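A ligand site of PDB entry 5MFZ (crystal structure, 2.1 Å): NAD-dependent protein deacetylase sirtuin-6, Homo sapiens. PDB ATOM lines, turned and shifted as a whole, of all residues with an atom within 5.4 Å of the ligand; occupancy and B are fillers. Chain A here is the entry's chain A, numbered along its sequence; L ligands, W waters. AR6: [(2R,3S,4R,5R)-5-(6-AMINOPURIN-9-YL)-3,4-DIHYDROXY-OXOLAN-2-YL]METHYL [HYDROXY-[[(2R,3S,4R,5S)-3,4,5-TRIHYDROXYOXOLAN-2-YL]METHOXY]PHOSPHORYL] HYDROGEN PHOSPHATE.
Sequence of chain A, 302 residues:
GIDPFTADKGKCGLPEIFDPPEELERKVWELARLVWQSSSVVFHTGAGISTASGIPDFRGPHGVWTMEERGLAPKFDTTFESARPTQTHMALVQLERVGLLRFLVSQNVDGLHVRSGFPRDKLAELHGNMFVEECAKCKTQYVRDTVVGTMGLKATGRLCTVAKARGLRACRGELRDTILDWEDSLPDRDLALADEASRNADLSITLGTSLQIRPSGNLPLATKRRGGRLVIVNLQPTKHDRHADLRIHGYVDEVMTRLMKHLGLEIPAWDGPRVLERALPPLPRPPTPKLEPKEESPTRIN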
ATOM      1  N   GLU A  16      22.006   8.909  13.395  1.00  0.00           N
ATOM      2  CA  GLU A  16      21.462   8.358  14.622  1.00  0.00           C
ATOM      3  C   GLU A  16      21.379   6.876  14.397  1.00  0.00           C
ATOM      4  O   GLU A  16      21.139   6.471  13.301  1.00  0.00           O
ATOM      5  CB  GLU A  16      20.077   8.903  14.913  1.00  0.00           C
ATOM      6  CG  GLU A  16      20.098  10.330  15.413  1.00  0.00           C
ATOM      7  CD  GLU A  16      18.740  10.805  15.780  1.00  0.00           C
ATOM      8  OE1 GLU A  16      17.757  10.407  15.159  1.00  0.00           O
ATOM      9  OE2 GLU A  16      18.651  11.580  16.751  1.00  0.00           O
ATOM     10  N   THR A  45      25.976  12.888  32.477  1.00  0.00           N
ATOM     11  CA  THR A  45      24.887  13.279  31.559  1.00  0.00           C
ATOM     12  C   THR A  45      25.325  14.472  30.634  1.00  0.00           C
ATOM     13  O   THR A  45      26.103  15.321  31.059  1.00  0.00           O
ATOM     14  CB  THR A  45      23.659  13.710  32.285  1.00  0.00           C
ATOM     15  OG1 THR A  45      24.036  14.837  33.141  1.00  0.00           O
ATOM     16  CG2 THR A  45      23.143  12.575  33.057  1.00  0.00           C
ATOM     17  N   GLY A  46      24.759  14.503  29.445  1.00  0.00           N
ATOM     18  CA  GLY A  46      24.845  15.668  28.556  1.00  0.00           C
ATOM     19  C   GLY A  46      23.497  16.038  27.985  1.00  0.00           C
ATOM     20  O   GLY A  46      22.449  15.540  28.430  1.00  0.00           O
ATOM     21  N   ALA A  47      23.537  16.808  26.906  1.00  0.00           N
ATOM     22  CA  ALA A  47      22.466  17.605  26.466  1.00  0.00           C
ATOM     23  C   ALA A  47      21.346  16.867  25.931  1.00  0.00           C
ATOM     24  O   ALA A  47      20.206  17.324  25.924  1.00  0.00           O
ATOM     25  CB  ALA A  47      23.007  18.678  25.471  1.00  0.00           C
ATOM     26  N   GLY A  48      21.607  15.623  25.510  1.00  0.00           N
ATOM     27  CA  GLY A  48      20.558  14.770  25.031  1.00  0.00           C
ATOM     28  C   GLY A  48      19.595  14.330  26.103  1.00  0.00           C
ATOM     29  O   GLY A  48      18.501  13.967  25.757  1.00  0.00           O
ATOM     30  N   ILE A  49      19.892  14.463  27.406  1.00  0.00           N
ATOM     31  CA  ILE A  49      18.806  14.098  28.449  1.00  0.00           C
ATOM     32  C   ILE A  49      17.726  15.151  28.569  1.00  0.00           C
ATOM     33  O   ILE A  49      16.784  14.989  29.350  1.00  0.00           O
ATOM     34  CB  ILE A  49      19.301  13.774  29.840  1.00  0.00           C
ATOM     35  CG1 ILE A  49      19.978  14.928  30.554  1.00  0.00           C
ATOM     36  CG2 ILE A  49      20.185  12.541  29.819  1.00  0.00           C
ATOM     37  CD1 ILE A  49      19.961  14.701  32.080  1.00  0.00           C
ATOM     38  N   THR A  51      16.555  17.057  25.616  1.00  0.00           N
ATOM     39  CA  THR A  51      15.855  17.288  24.356  1.00  0.00           C
ATOM     40  C   THR A  51      14.399  16.960  24.486  1.00  0.00           C
ATOM     41  O   THR A  51      13.560  17.588  23.787  1.00  0.00           O
ATOM     42  CB  THR A  51      16.503  16.445  23.166  1.00  0.00           C
ATOM     43  OG1 THR A  51      16.676  15.041  23.520  1.00  0.00           O
ATOM     44  CG2 THR A  51      17.807  16.998  22.851  1.00  0.00           C
ATOM     45  N   ALA A  52      14.028  15.928  25.284  1.00  0.00           N
ATOM     46  CA  ALA A  52      12.558  15.594  25.422  1.00  0.00           C
ATOM     47  C   ALA A  52      11.784  16.593  26.303  1.00  0.00           C
ATOM     48  O   ALA A  52      10.629  16.588  26.371  1.00  0.00           O
ATOM     49  CB  ALA A  52      12.375  14.176  25.970  1.00  0.00           C
ATOM     50  N   ASP A  57      19.932  19.808  21.732  1.00  0.00           N
ATOM     51  CA  ASP A  57      21.290  19.475  22.024  1.00  0.00           C
ATOM     52  C   ASP A  57      22.256  20.336  21.112  1.00  0.00           C
ATOM     53  O   ASP A  57      21.822  21.298  20.441  1.00  0.00           O
ATOM     54  CB  ASP A  57      21.546  17.962  21.979  1.00  0.00           C
ATOM     55  CG  ASP A  57      21.296  17.353  20.609  1.00  0.00           C
ATOM     56  OD1 ASP A  57      21.356  18.115  19.660  1.00  0.00           O
ATOM     57  OD2 ASP A  57      21.056  16.145  20.482  1.00  0.00           O
ATOM     58  N   PHE A  58      23.532  19.998  21.191  1.00  0.00           N
ATOM     59  CA  PHE A  58      24.580  20.683  20.494  1.00  0.00           C
ATOM     60  C   PHE A  58      24.947  20.042  19.140  1.00  0.00           C
ATOM     61  O   PHE A  58      25.096  20.758  18.145  1.00  0.00           O
ATOM     62  CB  PHE A  58      25.787  20.774  21.448  1.00  0.00           C
ATOM     63  CG  PHE A  58      25.551  21.788  22.571  1.00  0.00           C
ATOM     64  CD1 PHE A  58      25.661  23.119  22.353  1.00  0.00           C
ATOM     65  CD2 PHE A  58      25.190  21.339  23.865  1.00  0.00           C
ATOM     66  CE1 PHE A  58      25.426  24.039  23.363  1.00  0.00           C
ATOM     67  CE2 PHE A  58      25.025  22.238  24.892  1.00  0.00           C
ATOM     68  CZ  PHE A  58      25.114  23.591  24.644  1.00  0.00           C
ATOM     69  N   ARG A  59      25.074  18.709  19.116  1.00  0.00           N
ATOM     70  CA  ARG A  59      25.607  18.009  17.967  1.00  0.00           C
ATOM     71  C   ARG A  59      24.659  17.031  17.374  1.00  0.00           C
ATOM     72  O   ARG A  59      25.035  16.328  16.412  1.00  0.00           O
ATOM     73  CB  ARG A  59      27.013  17.355  18.269  1.00  0.00           C
ATOM     74  CG  ARG A  59      28.021  18.449  18.784  1.00  0.00           C
ATOM     75  CD  ARG A  59      29.395  17.903  19.169  1.00  0.00           C
ATOM     76  NE  ARG A  59      30.202  18.940  19.802  1.00  0.00           N
ATOM     77  CZ  ARG A  59      30.064  19.395  21.056  1.00  0.00           C
ATOM     78  NH1 ARG A  59      29.277  18.799  21.919  1.00  0.00           N
ATOM     79  NH2 ARG A  59      30.850  20.363  21.520  1.00  0.00           N
ATOM     80  N   GLY A  60      23.420  17.027  17.837  1.00  0.00           N
ATOM     81  CA  GLY A  60      22.402  16.149  17.265  1.00  0.00           C
ATOM     82  C   GLY A  60      22.044  16.597  15.840  1.00  0.00           C
ATOM     83  O   GLY A  60      22.408  17.684  15.427  1.00  0.00           O
ATOM     84  N   PRO A  61      21.160  15.862  15.167  1.00  0.00           N
ATOM     85  CA  PRO A  61      20.764  16.339  13.900  1.00  0.00           C
ATOM     86  C   PRO A  61      20.221  17.756  13.839  1.00  0.00           C
ATOM     87  O   PRO A  61      20.357  18.407  12.782  1.00  0.00           O
ATOM     88  CB  PRO A  61      19.665  15.343  13.456  1.00  0.00           C
ATOM     89  CG  PRO A  61      19.777  14.222  14.313  1.00  0.00           C
ATOM     90  CD  PRO A  61      20.280  14.772  15.613  1.00  0.00           C
ATOM     91  N   TRP A  65      25.064  23.584  17.362  1.00  0.00           N
ATOM     92  CA  TRP A  65      26.181  23.610  16.424  1.00  0.00           C
ATOM     93  C   TRP A  65      25.845  22.945  15.084  1.00  0.00           C
ATOM     94  O   TRP A  65      26.145  23.491  14.016  1.00  0.00           O
ATOM     95  CB  TRP A  65      27.472  23.045  17.002  1.00  0.00           C
ATOM     96  CG  TRP A  65      27.917  23.488  18.376  1.00  0.00           C
ATOM     97  CD1 TRP A  65      28.631  22.701  19.282  1.00  0.00           C
ATOM     98  CD2 TRP A  65      27.870  24.767  18.952  1.00  0.00           C
ATOM     99  NE1 TRP A  65      28.934  23.402  20.416  1.00  0.00           N
ATOM    100  CE2 TRP A  65      28.464  24.671  20.261  1.00  0.00           C
ATOM    101  CE3 TRP A  65      27.304  25.998  18.545  1.00  0.00           C
ATOM    102  CZ2 TRP A  65      28.504  25.724  21.121  1.00  0.00           C
ATOM    103  CZ3 TRP A  65      27.307  27.037  19.416  1.00  0.00           C
ATOM    104  CH2 TRP A  65      27.915  26.909  20.699  1.00  0.00           C
ATOM    105  N   GLN A 107      27.380  17.930  32.118  1.00  0.00           N
ATOM    106  CA  GLN A 107      27.959  18.933  31.322  1.00  0.00           C
ATOM    107  C   GLN A 107      26.886  19.972  31.053  1.00  0.00           C
ATOM    108  O   GLN A 107      27.181  20.955  30.334  1.00  0.00           O
ATOM    109  CB  GLN A 107      28.425  18.268  30.046  1.00  0.00           C
ATOM    110  CG  GLN A 107      29.730  17.493  30.222  1.00  0.00           C
ATOM    111  CD  GLN A 107      30.023  16.708  29.009  1.00  0.00           C
ATOM    112  OE1 GLN A 107      30.574  17.227  28.021  1.00  0.00           O
ATOM    113  NE2 GLN A 107      29.567  15.428  29.011  1.00  0.00           N
ATOM    114  N   ASN A 108      25.620  19.793  31.527  1.00  0.00           N
ATOM    115  CA  ASN A 108      24.539  20.632  31.053  1.00  0.00           C
ATOM    116  C   ASN A 108      24.577  21.827  31.948  1.00  0.00           C
ATOM    117  O   ASN A 108      24.798  21.722  33.136  1.00  0.00           O
ATOM    118  CB  ASN A 108      23.223  19.923  31.167  1.00  0.00           C
ATOM    119  CG  ASN A 108      23.224  18.693  30.363  1.00  0.00           C
ATOM    120  OD1 ASN A 108      24.035  18.623  29.463  1.00  0.00           O
ATOM    121  ND2 ASN A 108      22.355  17.753  30.636  1.00  0.00           N
ATOM    122  N   HIS A 127      30.094  22.516  33.532  1.00  0.00           N
ATOM    123  CA  HIS A 127      30.188  23.645  32.602  1.00  0.00           C
ATOM    124  C   HIS A 127      29.475  24.845  33.138  1.00  0.00           C
ATOM    125  O   HIS A 127      29.337  25.774  32.394  1.00  0.00           O
ATOM    126  CB  HIS A 127      29.734  23.253  31.191  1.00  0.00           C
ATOM    127  CG  HIS A 127      30.563  22.193  30.570  1.00  0.00           C
ATOM    128  ND1 HIS A 127      30.161  21.449  29.467  1.00  0.00           N
ATOM    129  CD2 HIS A 127      31.765  21.681  30.945  1.00  0.00           C
ATOM    130  CE1 HIS A 127      31.069  20.549  29.193  1.00  0.00           C
ATOM    131  NE2 HIS A 127      32.042  20.659  30.078  1.00  0.00           N
ATOM    132  N   TRP A 182      34.566  29.267  26.083  1.00  0.00           N
ATOM    133  CA  TRP A 182      35.578  28.429  25.387  1.00  0.00           C
ATOM    134  C   TRP A 182      36.942  28.328  26.056  1.00  0.00           C
ATOM    135  O   TRP A 182      37.497  27.199  26.147  1.00  0.00           O
ATOM    136  CB  TRP A 182      35.734  28.816  23.895  1.00  0.00           C
ATOM    137  CG  TRP A 182      34.547  28.350  23.149  1.00  0.00           C
ATOM    138  CD1 TRP A 182      33.462  29.128  22.745  1.00  0.00           C
ATOM    139  CD2 TRP A 182      34.194  26.975  22.827  1.00  0.00           C
ATOM    140  NE1 TRP A 182      32.489  28.305  22.160  1.00  0.00           N
ATOM    141  CE2 TRP A 182      32.908  26.994  22.215  1.00  0.00           C
ATOM    142  CE3 TRP A 182      34.840  25.739  23.002  1.00  0.00           C
ATOM    143  CZ2 TRP A 182      32.266  25.810  21.753  1.00  0.00           C
ATOM    144  CZ3 TRP A 182      34.186  24.538  22.518  1.00  0.00           C
ATOM    145  CH2 TRP A 182      32.940  24.596  21.909  1.00  0.00           C
ATOM    146  N   GLY A 208      23.090  10.554  26.848  1.00  0.00           N
ATOM    147  CA  GLY A 208      22.901  11.800  26.022  1.00  0.00           C
ATOM    148  C   GLY A 208      24.081  12.735  25.965  1.00  0.00           C
ATOM    149  O   GLY A 208      23.902  13.950  26.001  1.00  0.00           O
ATOM    150  N   THR A 209      25.296  12.171  25.991  1.00  0.00           N
ATOM    151  CA  THR A 209      26.486  12.863  25.591  1.00  0.00           C
ATOM    152  C   THR A 209      27.376  12.151  24.529  1.00  0.00           C
ATOM    153  O   THR A 209      27.551  10.899  24.506  1.00  0.00           O
ATOM    154  CB  THR A 209      27.304  13.210  26.824  1.00  0.00           C
ATOM    155  OG1 THR A 209      28.477  13.872  26.394  1.00  0.00           O
ATOM    156  CG2 THR A 209      27.656  11.991  27.620  1.00  0.00           C
ATOM    157  N   SER A 210      27.879  12.939  23.562  1.00  0.00           N
ATOM    158  CA  SER A 210      28.635  12.421  22.502  1.00  0.00           C
ATOM    159  C   SER A 210      30.090  12.423  22.949  1.00  0.00           C
ATOM    160  O   SER A 210      30.969  11.921  22.232  1.00  0.00           O
ATOM    161  CB  SER A 210      28.418  13.282  21.221  1.00  0.00           C
ATOM    162  OG  SER A 210      29.023  14.563  21.381  1.00  0.00           O
ATOM    163  N   LEU A 211      30.333  12.817  24.192  1.00  0.00           N
ATOM    164  CA  LEU A 211      31.687  12.614  24.874  1.00  0.00           C
ATOM    165  C   LEU A 211      32.886  13.236  24.190  1.00  0.00           C
ATOM    166  O   LEU A 211      34.067  12.942  24.455  1.00  0.00           O
ATOM    167  CB  LEU A 211      31.957  11.066  25.179  1.00  0.00           C
ATOM    168  CG  LEU A 211      30.952  10.369  26.030  1.00  0.00           C
ATOM    169  CD1 LEU A 211      31.168   8.883  26.050  1.00  0.00           C
ATOM    170  CD2 LEU A 211      30.944  10.902  27.477  1.00  0.00           C
ATOM    171  N   GLN A 212      32.613  14.224  23.395  1.00  0.00           N
ATOM    172  CA  GLN A 212      33.702  14.891  22.630  1.00  0.00           C
ATOM    173  C   GLN A 212      34.508  15.945  23.338  1.00  0.00           C
ATOM    174  O   GLN A 212      35.497  16.337  22.791  1.00  0.00           O
ATOM    175  CB  GLN A 212      33.091  15.492  21.414  1.00  0.00           C
ATOM    176  CG  GLN A 212      32.541  14.456  20.441  1.00  0.00           C
ATOM    177  CD  GLN A 212      32.065  15.105  19.185  1.00  0.00           C
ATOM    178  OE1 GLN A 212      32.857  15.767  18.626  1.00  0.00           O
ATOM    179  NE2 GLN A 212      30.832  14.871  18.688  1.00  0.00           N
ATOM    180  N   ILE A 213      34.056  16.473  24.476  1.00  0.00           N
ATOM    181  CA  ILE A 213      34.729  17.552  25.159  1.00  0.00           C
ATOM    182  C   ILE A 213      35.614  16.958  26.171  1.00  0.00           C
ATOM    183  O   ILE A 213      35.185  16.069  26.908  1.00  0.00           O
ATOM    184  CB  ILE A 213      33.719  18.489  25.863  1.00  0.00           C
ATOM    185  CG1 ILE A 213      32.900  19.219  24.804  1.00  0.00           C
ATOM    186  CG2 ILE A 213      34.425  19.478  26.809  1.00  0.00           C
ATOM    187  CD1 ILE A 213      33.676  20.294  24.023  1.00  0.00           C
ATOM    188  N   VAL A 233      24.817   5.363  26.611  1.00  0.00           N
ATOM    189  CA  VAL A 233      23.420   5.356  26.134  1.00  0.00           C
ATOM    190  C   VAL A 233      23.367   6.605  25.323  1.00  0.00           C
ATOM    191  O   VAL A 233      23.596   7.688  25.870  1.00  0.00           O
ATOM    192  CB  VAL A 233      22.399   5.351  27.273  1.00  0.00           C
ATOM    193  CG1 VAL A 233      21.001   5.189  26.694  1.00  0.00           C
ATOM    194  CG2 VAL A 233      22.604   4.150  28.228  1.00  0.00           C
ATOM    195  N   ASN A 234      23.164   6.479  24.002  1.00  0.00           N
ATOM    196  CA  ASN A 234      23.184   7.632  23.063  1.00  0.00           C
ATOM    197  C   ASN A 234      22.630   7.218  21.709  1.00  0.00           C
ATOM    198  O   ASN A 234      22.877   6.101  21.254  1.00  0.00           O
ATOM    199  CB  ASN A 234      24.600   8.105  22.880  1.00  0.00           C
ATOM    200  CG  ASN A 234      24.702   9.599  22.581  1.00  0.00           C
ATOM    201  OD1 ASN A 234      24.210  10.443  23.315  1.00  0.00           O
ATOM    202  ND2 ASN A 234      25.384   9.932  21.494  1.00  0.00           N
ATOM    203  N   LEU A 235      21.851   8.093  21.090  1.00  0.00           N
ATOM    204  CA  LEU A 235      21.368   7.917  19.766  1.00  0.00           C
ATOM    205  C   LEU A 235      22.479   7.972  18.613  1.00  0.00           C
ATOM    206  O   LEU A 235      22.461   7.201  17.685  1.00  0.00           O
ATOM    207  CB  LEU A 235      20.316   8.976  19.497  1.00  0.00           C
ATOM    208  CG  LEU A 235      18.946   8.696  20.047  1.00  0.00           C
ATOM    209  CD1 LEU A 235      18.072   9.906  19.800  1.00  0.00           C
ATOM    210  CD2 LEU A 235      18.419   7.458  19.378  1.00  0.00           C
ATOM    211  N   GLN A 236      23.438   8.868  18.716  1.00  0.00           N
ATOM    212  CA  GLN A 236      24.563   8.950  17.876  1.00  0.00           C
ATOM    213  C   GLN A 236      25.769   8.132  18.411  1.00  0.00           C
ATOM    214  O   GLN A 236      25.920   7.828  19.589  1.00  0.00           O
ATOM    215  CB  GLN A 236      25.048  10.399  17.760  1.00  0.00           C
ATOM    216  CG  GLN A 236      24.122  11.280  17.000  1.00  0.00           C
ATOM    217  CD  GLN A 236      24.590  12.733  16.922  1.00  0.00           C
ATOM    218  OE1 GLN A 236      25.279  13.244  17.749  1.00  0.00           O
ATOM    219  NE2 GLN A 236      24.159  13.380  15.910  1.00  0.00           N
ATOM    220  N   PRO A 237      26.724   7.875  17.535  1.00  0.00           N
ATOM    221  CA  PRO A 237      28.042   7.461  18.005  1.00  0.00           C
ATOM    222  C   PRO A 237      28.639   8.517  18.839  1.00  0.00           C
ATOM    223  O   PRO A 237      28.241   9.649  18.738  1.00  0.00           O
ATOM    224  CB  PRO A 237      28.864   7.294  16.693  1.00  0.00           C
ATOM    225  CG  PRO A 237      27.910   7.523  15.539  1.00  0.00           C
ATOM    226  CD  PRO A 237      26.601   8.039  16.064  1.00  0.00           C
ATOM    227  N   GLY A 250      19.239   4.186  21.853  1.00  0.00           N
ATOM    228  CA  GLY A 250      17.836   4.496  22.020  1.00  0.00           C
ATOM    229  C   GLY A 250      17.592   5.809  22.667  1.00  0.00           C
ATOM    230  O   GLY A 250      18.529   6.508  23.074  1.00  0.00           O
ATOM    231  N   TYR A 251      16.323   6.173  22.720  1.00  0.00           N
ATOM    232  CA  TYR A 251      15.923   7.347  23.445  1.00  0.00           C
ATOM    233  C   TYR A 251      16.138   7.107  24.967  1.00  0.00           C
ATOM    234  O   TYR A 251      15.731   6.047  25.501  1.00  0.00           O
ATOM    235  CB  TYR A 251      14.454   7.597  23.219  1.00  0.00           C
ATOM    236  CG  TYR A 251      14.187   8.082  21.832  1.00  0.00           C
ATOM    237  CD1 TYR A 251      14.543   9.355  21.458  1.00  0.00           C
ATOM    238  CD2 TYR A 251      13.588   7.256  20.893  1.00  0.00           C
ATOM    239  CE1 TYR A 251      14.292   9.796  20.190  1.00  0.00           C
ATOM    240  CE2 TYR A 251      13.307   7.679  19.595  1.00  0.00           C
ATOM    241  CZ  TYR A 251      13.662   8.931  19.253  1.00  0.00           C
ATOM    242  OH  TYR A 251      13.444   9.378  18.009  1.00  0.00           O
ATOM    243  N   VAL A 252      16.821   8.037  25.622  1.00  0.00           N
ATOM    244  CA  VAL A 252      17.150   7.830  27.029  1.00  0.00           C
ATOM    245  C   VAL A 252      15.943   7.686  27.939  1.00  0.00           C
ATOM    246  O   VAL A 252      15.959   6.816  28.756  1.00  0.00           O
ATOM    247  CB  VAL A 252      18.034   8.882  27.633  1.00  0.00           C
ATOM    248  CG1 VAL A 252      19.380   8.737  27.022  1.00  0.00           C
ATOM    249  CG2 VAL A 252      17.433  10.324  27.477  1.00  0.00           C
ATOM    250  N   ASP A 253      14.867   8.386  27.676  1.00  0.00           N
ATOM    251  CA  ASP A 253      13.645   8.213  28.473  1.00  0.00           C
ATOM    252  C   ASP A 253      13.127   6.806  28.311  1.00  0.00           C
ATOM    253  O   ASP A 253      12.632   6.269  29.297  1.00  0.00           O
ATOM    254  CB  ASP A 253      12.503   9.195  28.172  1.00  0.00           C
ATOM    255  CG  ASP A 253      12.771  10.572  28.688  1.00  0.00           C
ATOM    256  OD1 ASP A 253      13.727  10.795  29.496  1.00  0.00           O
ATOM    257  OD2 ASP A 253      11.990  11.437  28.248  1.00  0.00           O
HETATM  258  N1  AR6 L   1      17.986   9.949  23.802  1.00  0.00           N
HETATM  259  C2  AR6 L   1      19.248   9.544  23.573  1.00  0.00           C
HETATM  260  N3  AR6 L   1      20.227  10.269  23.027  1.00  0.00           N
HETATM  261  C4  AR6 L   1      19.964  11.589  22.713  1.00  0.00           C
HETATM  262  C5  AR6 L   1      18.625  12.101  22.804  1.00  0.00           C
HETATM  263  C6  AR6 L   1      17.623  11.212  23.452  1.00  0.00           C
HETATM  264  N6  AR6 L   1      16.408  11.736  23.607  1.00  0.00           N
HETATM  265  N7  AR6 L   1      18.650  13.322  22.321  1.00  0.00           N
HETATM  266  C8  AR6 L   1      19.877  13.614  21.971  1.00  0.00           C
HETATM  267  N9  AR6 L   1      20.654  12.555  22.171  1.00  0.00           N
HETATM  268  PA  AR6 L   1      26.133  16.830  22.322  1.00  0.00           P
HETATM  269  PB  AR6 L   1      27.201  17.166  25.013  1.00  0.00           P
HETATM  270  C1' AR6 L   1      22.094  12.430  21.817  1.00  0.00           C
HETATM  271  O1A AR6 L   1      27.542  16.821  21.897  1.00  0.00           O
HETATM  272  O1B AR6 L   1      26.321  17.222  26.298  1.00  0.00           O
HETATM  273  C1D AR6 L   1      29.020  21.914  24.095  1.00  0.00           C
HETATM  274  O1D AR6 L   1      29.961  22.746  23.395  1.00  0.00           O
HETATM  275  C2' AR6 L   1      22.619  12.996  20.505  1.00  0.00           C
HETATM  276  O2' AR6 L   1      22.559  11.958  19.537  1.00  0.00           O
HETATM  277  O2A AR6 L   1      24.922  17.315  21.545  1.00  0.00           O
HETATM  278  O2B AR6 L   1      27.999  15.849  24.975  1.00  0.00           O
HETATM  279  C2D AR6 L   1      28.558  22.374  25.515  1.00  0.00           C
HETATM  280  O2D AR6 L   1      29.712  22.899  26.151  1.00  0.00           O
HETATM  281  C3' AR6 L   1      24.059  13.442  20.848  1.00  0.00           C
HETATM  282  O3' AR6 L   1      25.161  12.570  20.524  1.00  0.00           O
HETATM  283  O3A AR6 L   1      26.076  17.388  23.853  1.00  0.00           O
HETATM  284  C3D AR6 L   1      28.241  21.012  26.213  1.00  0.00           C
HETATM  285  O3D AR6 L   1      28.312  21.081  27.696  1.00  0.00           O
HETATM  286  C4' AR6 L   1      24.096  13.481  22.386  1.00  0.00           C
HETATM  287  O4' AR6 L   1      22.727  13.242  22.755  1.00  0.00           O
HETATM  288  C4D AR6 L   1      29.358  20.158  25.677  1.00  0.00           C
HETATM  289  O4D AR6 L   1      29.725  20.674  24.335  1.00  0.00           O
HETATM  290  C5' AR6 L   1      24.360  14.862  22.911  1.00  0.00           C
HETATM  291  O5' AR6 L   1      25.702  15.284  22.479  1.00  0.00           O
HETATM  292  C5D AR6 L   1      29.237  18.667  25.567  1.00  0.00           C
HETATM  293  O5D AR6 L   1      28.066  18.409  24.780  1.00  0.00           O
HETATM  294  O   HOH W   1      15.727  13.600  26.082  1.00  0.00           O
HETATM  295  O   HOH W   2      14.613  10.796  25.857  1.00  0.00           O
HETATM  296  O   HOH W   3      20.549  12.506  17.954  1.00  0.00           O
HETATM  297  O   HOH W   4      25.924  19.703  27.657  1.00  0.00           O
HETATM  298  O   HOH W   5      30.331  15.932  23.448  1.00  0.00           O
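The side-chain hydroxyl (OG) of Ser 210 lies within hydrogen-bond range of an oxygen (O1A) of the ligand (2.7 Å). O2A of the ligand lies within hydrogen-bond range of N of Arg 59, at 2.8 Å. O2A of the ligand is in hydrogen-bond range of N of Phe 58, at 3.0 Å. ND1 of His 127 sits at hydrogen-bond distance from O3D of the ligand (2.6 Å). A nitrogen (N7) of the ligand sits at hydrogen-bond distance from the side-chain hydroxyl (OG1) of Thr 51 (2.9 Å). The side-chain amide oxygen (OE1) of Gln 236 is in hydrogen-bond range of an oxygen (O3') of the ligand (2.9 Å). A nitrogen (N1) of the ligand is in hydrogen-bond range of the backbone NH of Val 252, 2.9 Å away. The guanidinium group (NH1) of Arg 59 lies within salt-bridge range of an oxygen (O1A) of the ligand. The backbone NH (N) of Ser 210 is in hydrogen-bond range of an oxygen (O2B) of the ligand. The backbone carbonyl oxygen (O) of Gln 107 lies within hydrogen-bond range of an oxygen (O3D) of the ligand, at 2.9 Å. An oxygen (O1D) of the ligand is in hydrogen-bond range of the indole nitrogen (NE1) of Trp 65, at 3.2 Å. N of Leu 235 is in hydrogen-bond range of N3 of the ligand, at 3.3 Å. An oxygen (O1B) of the ligand is in hydrogen-bond range of the backbone NH (N) of Ala 47. The side-chain amide nitrogen of Asn 234 sits at hydrogen-bond distance from an oxygen (O3') of the ligand, 2.8 Å away. The side-chain hydroxyl (OG1) of Thr 209 sits at hydrogen-bond distance from an oxygen (O2B) of the ligand. N of Gln 236 lies close to O2' of the ligand.
The side-chain hydroxyl (OG) of Ser 210 sits at hydrogen-bond distance from the side-chain amide nitrogen (NE2) of Gln 212, at 3.3 Å. A ring nitrogen (ND1) of His 127 lies within hydrogen-bond range of the backbone carbonyl oxygen (O) of Gln 107, at 3.1 Å. The side-chain hydroxyl of Thr 209 lies close to the backbone NH of Leu 211, 3.1 Å away. The backbone carbonyl oxygen (O) of Val 233 sits at hydrogen-bond distance from the backbone NH (N) of Gly 208 (3.1 Å). The backbone NH of Thr 209 is in hydrogen-bond range of the side-chain amide oxygen of Asn 234, 3.4 Å away. The side-chain hydroxyl of Thr 51 sits at hydrogen-bond distance from the backbone carbonyl oxygen of Gly 48 (3.1 Å). The backbone NH of Ala 47 sits at hydrogen-bond distance from the backbone carbonyl oxygen of Gly 208 (3.0 Å). N of Gln 107 lies within hydrogen-bond range of O of Thr 45 (3.1 Å).
The backbone carbonyl oxygen (O) of Gly 48 lies close to a nitrogen (N7) of the ligand (3.5 Å). CA of Gly 46 touches O1B of the ligand, at 3.1 Å. OD2 of Asp 57 touches C8 of the ligand, 3.2 Å away. Trp 182 touches the ligand. O of Gly 208 touches C5' of the ligand (3.3 Å). Leu 211 touches the ligand (N to O2B, 3.9 Å). CG1 of Ile 213 touches O4D of the ligand, at 3.5 Å. Gly 250 touches the ligand (O to C2, 3.2 Å). Tyr 251 touches the ligand. Hydrophobic or aromatic side chains within 4 Å of the ligand: Ala 47, Phe 58, Trp 65, His 127, Trp 182, Ile 213, Leu 235, Tyr 251 and Val 252. 22 residues have an atom within 4 Å of the ligand: Gly 46, Ala 47, Gly 48, Thr 51, Asp 57, Phe 58, Arg 59, Trp 65, Gln 107, His 127, Trp 182, Gly 208, Thr 209, Ser 210, Leu 211, Ile 213, Asn 234, Leu 235, Gln 236, Gly 250, Tyr 251 and Val 252. The nearest printed residue that does not touch the ligand is Gly 60 (4.01 Å).
Water W3 bridges the side-chain carboxylate of Glu 16 (2.4 Å) and an oxygen (O2') of the ligand (2.6 Å). Water W4 lies within hydrogen-bond range of O3D of the ligand, OD1 of Asn 108 and O of Gln 107. Water W2 lies within hydrogen-bond range of N6 of the ligand (3.0 Å) and N of Asp 253 (3.0 Å). Water W1 lies within hydrogen-bond range of O of Gly 48 (2.8 Å), N of Ala 52 (3.0 Å), OG1 of Thr 51 (3.1 Å) and N6 of the ligand (3.2 Å).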
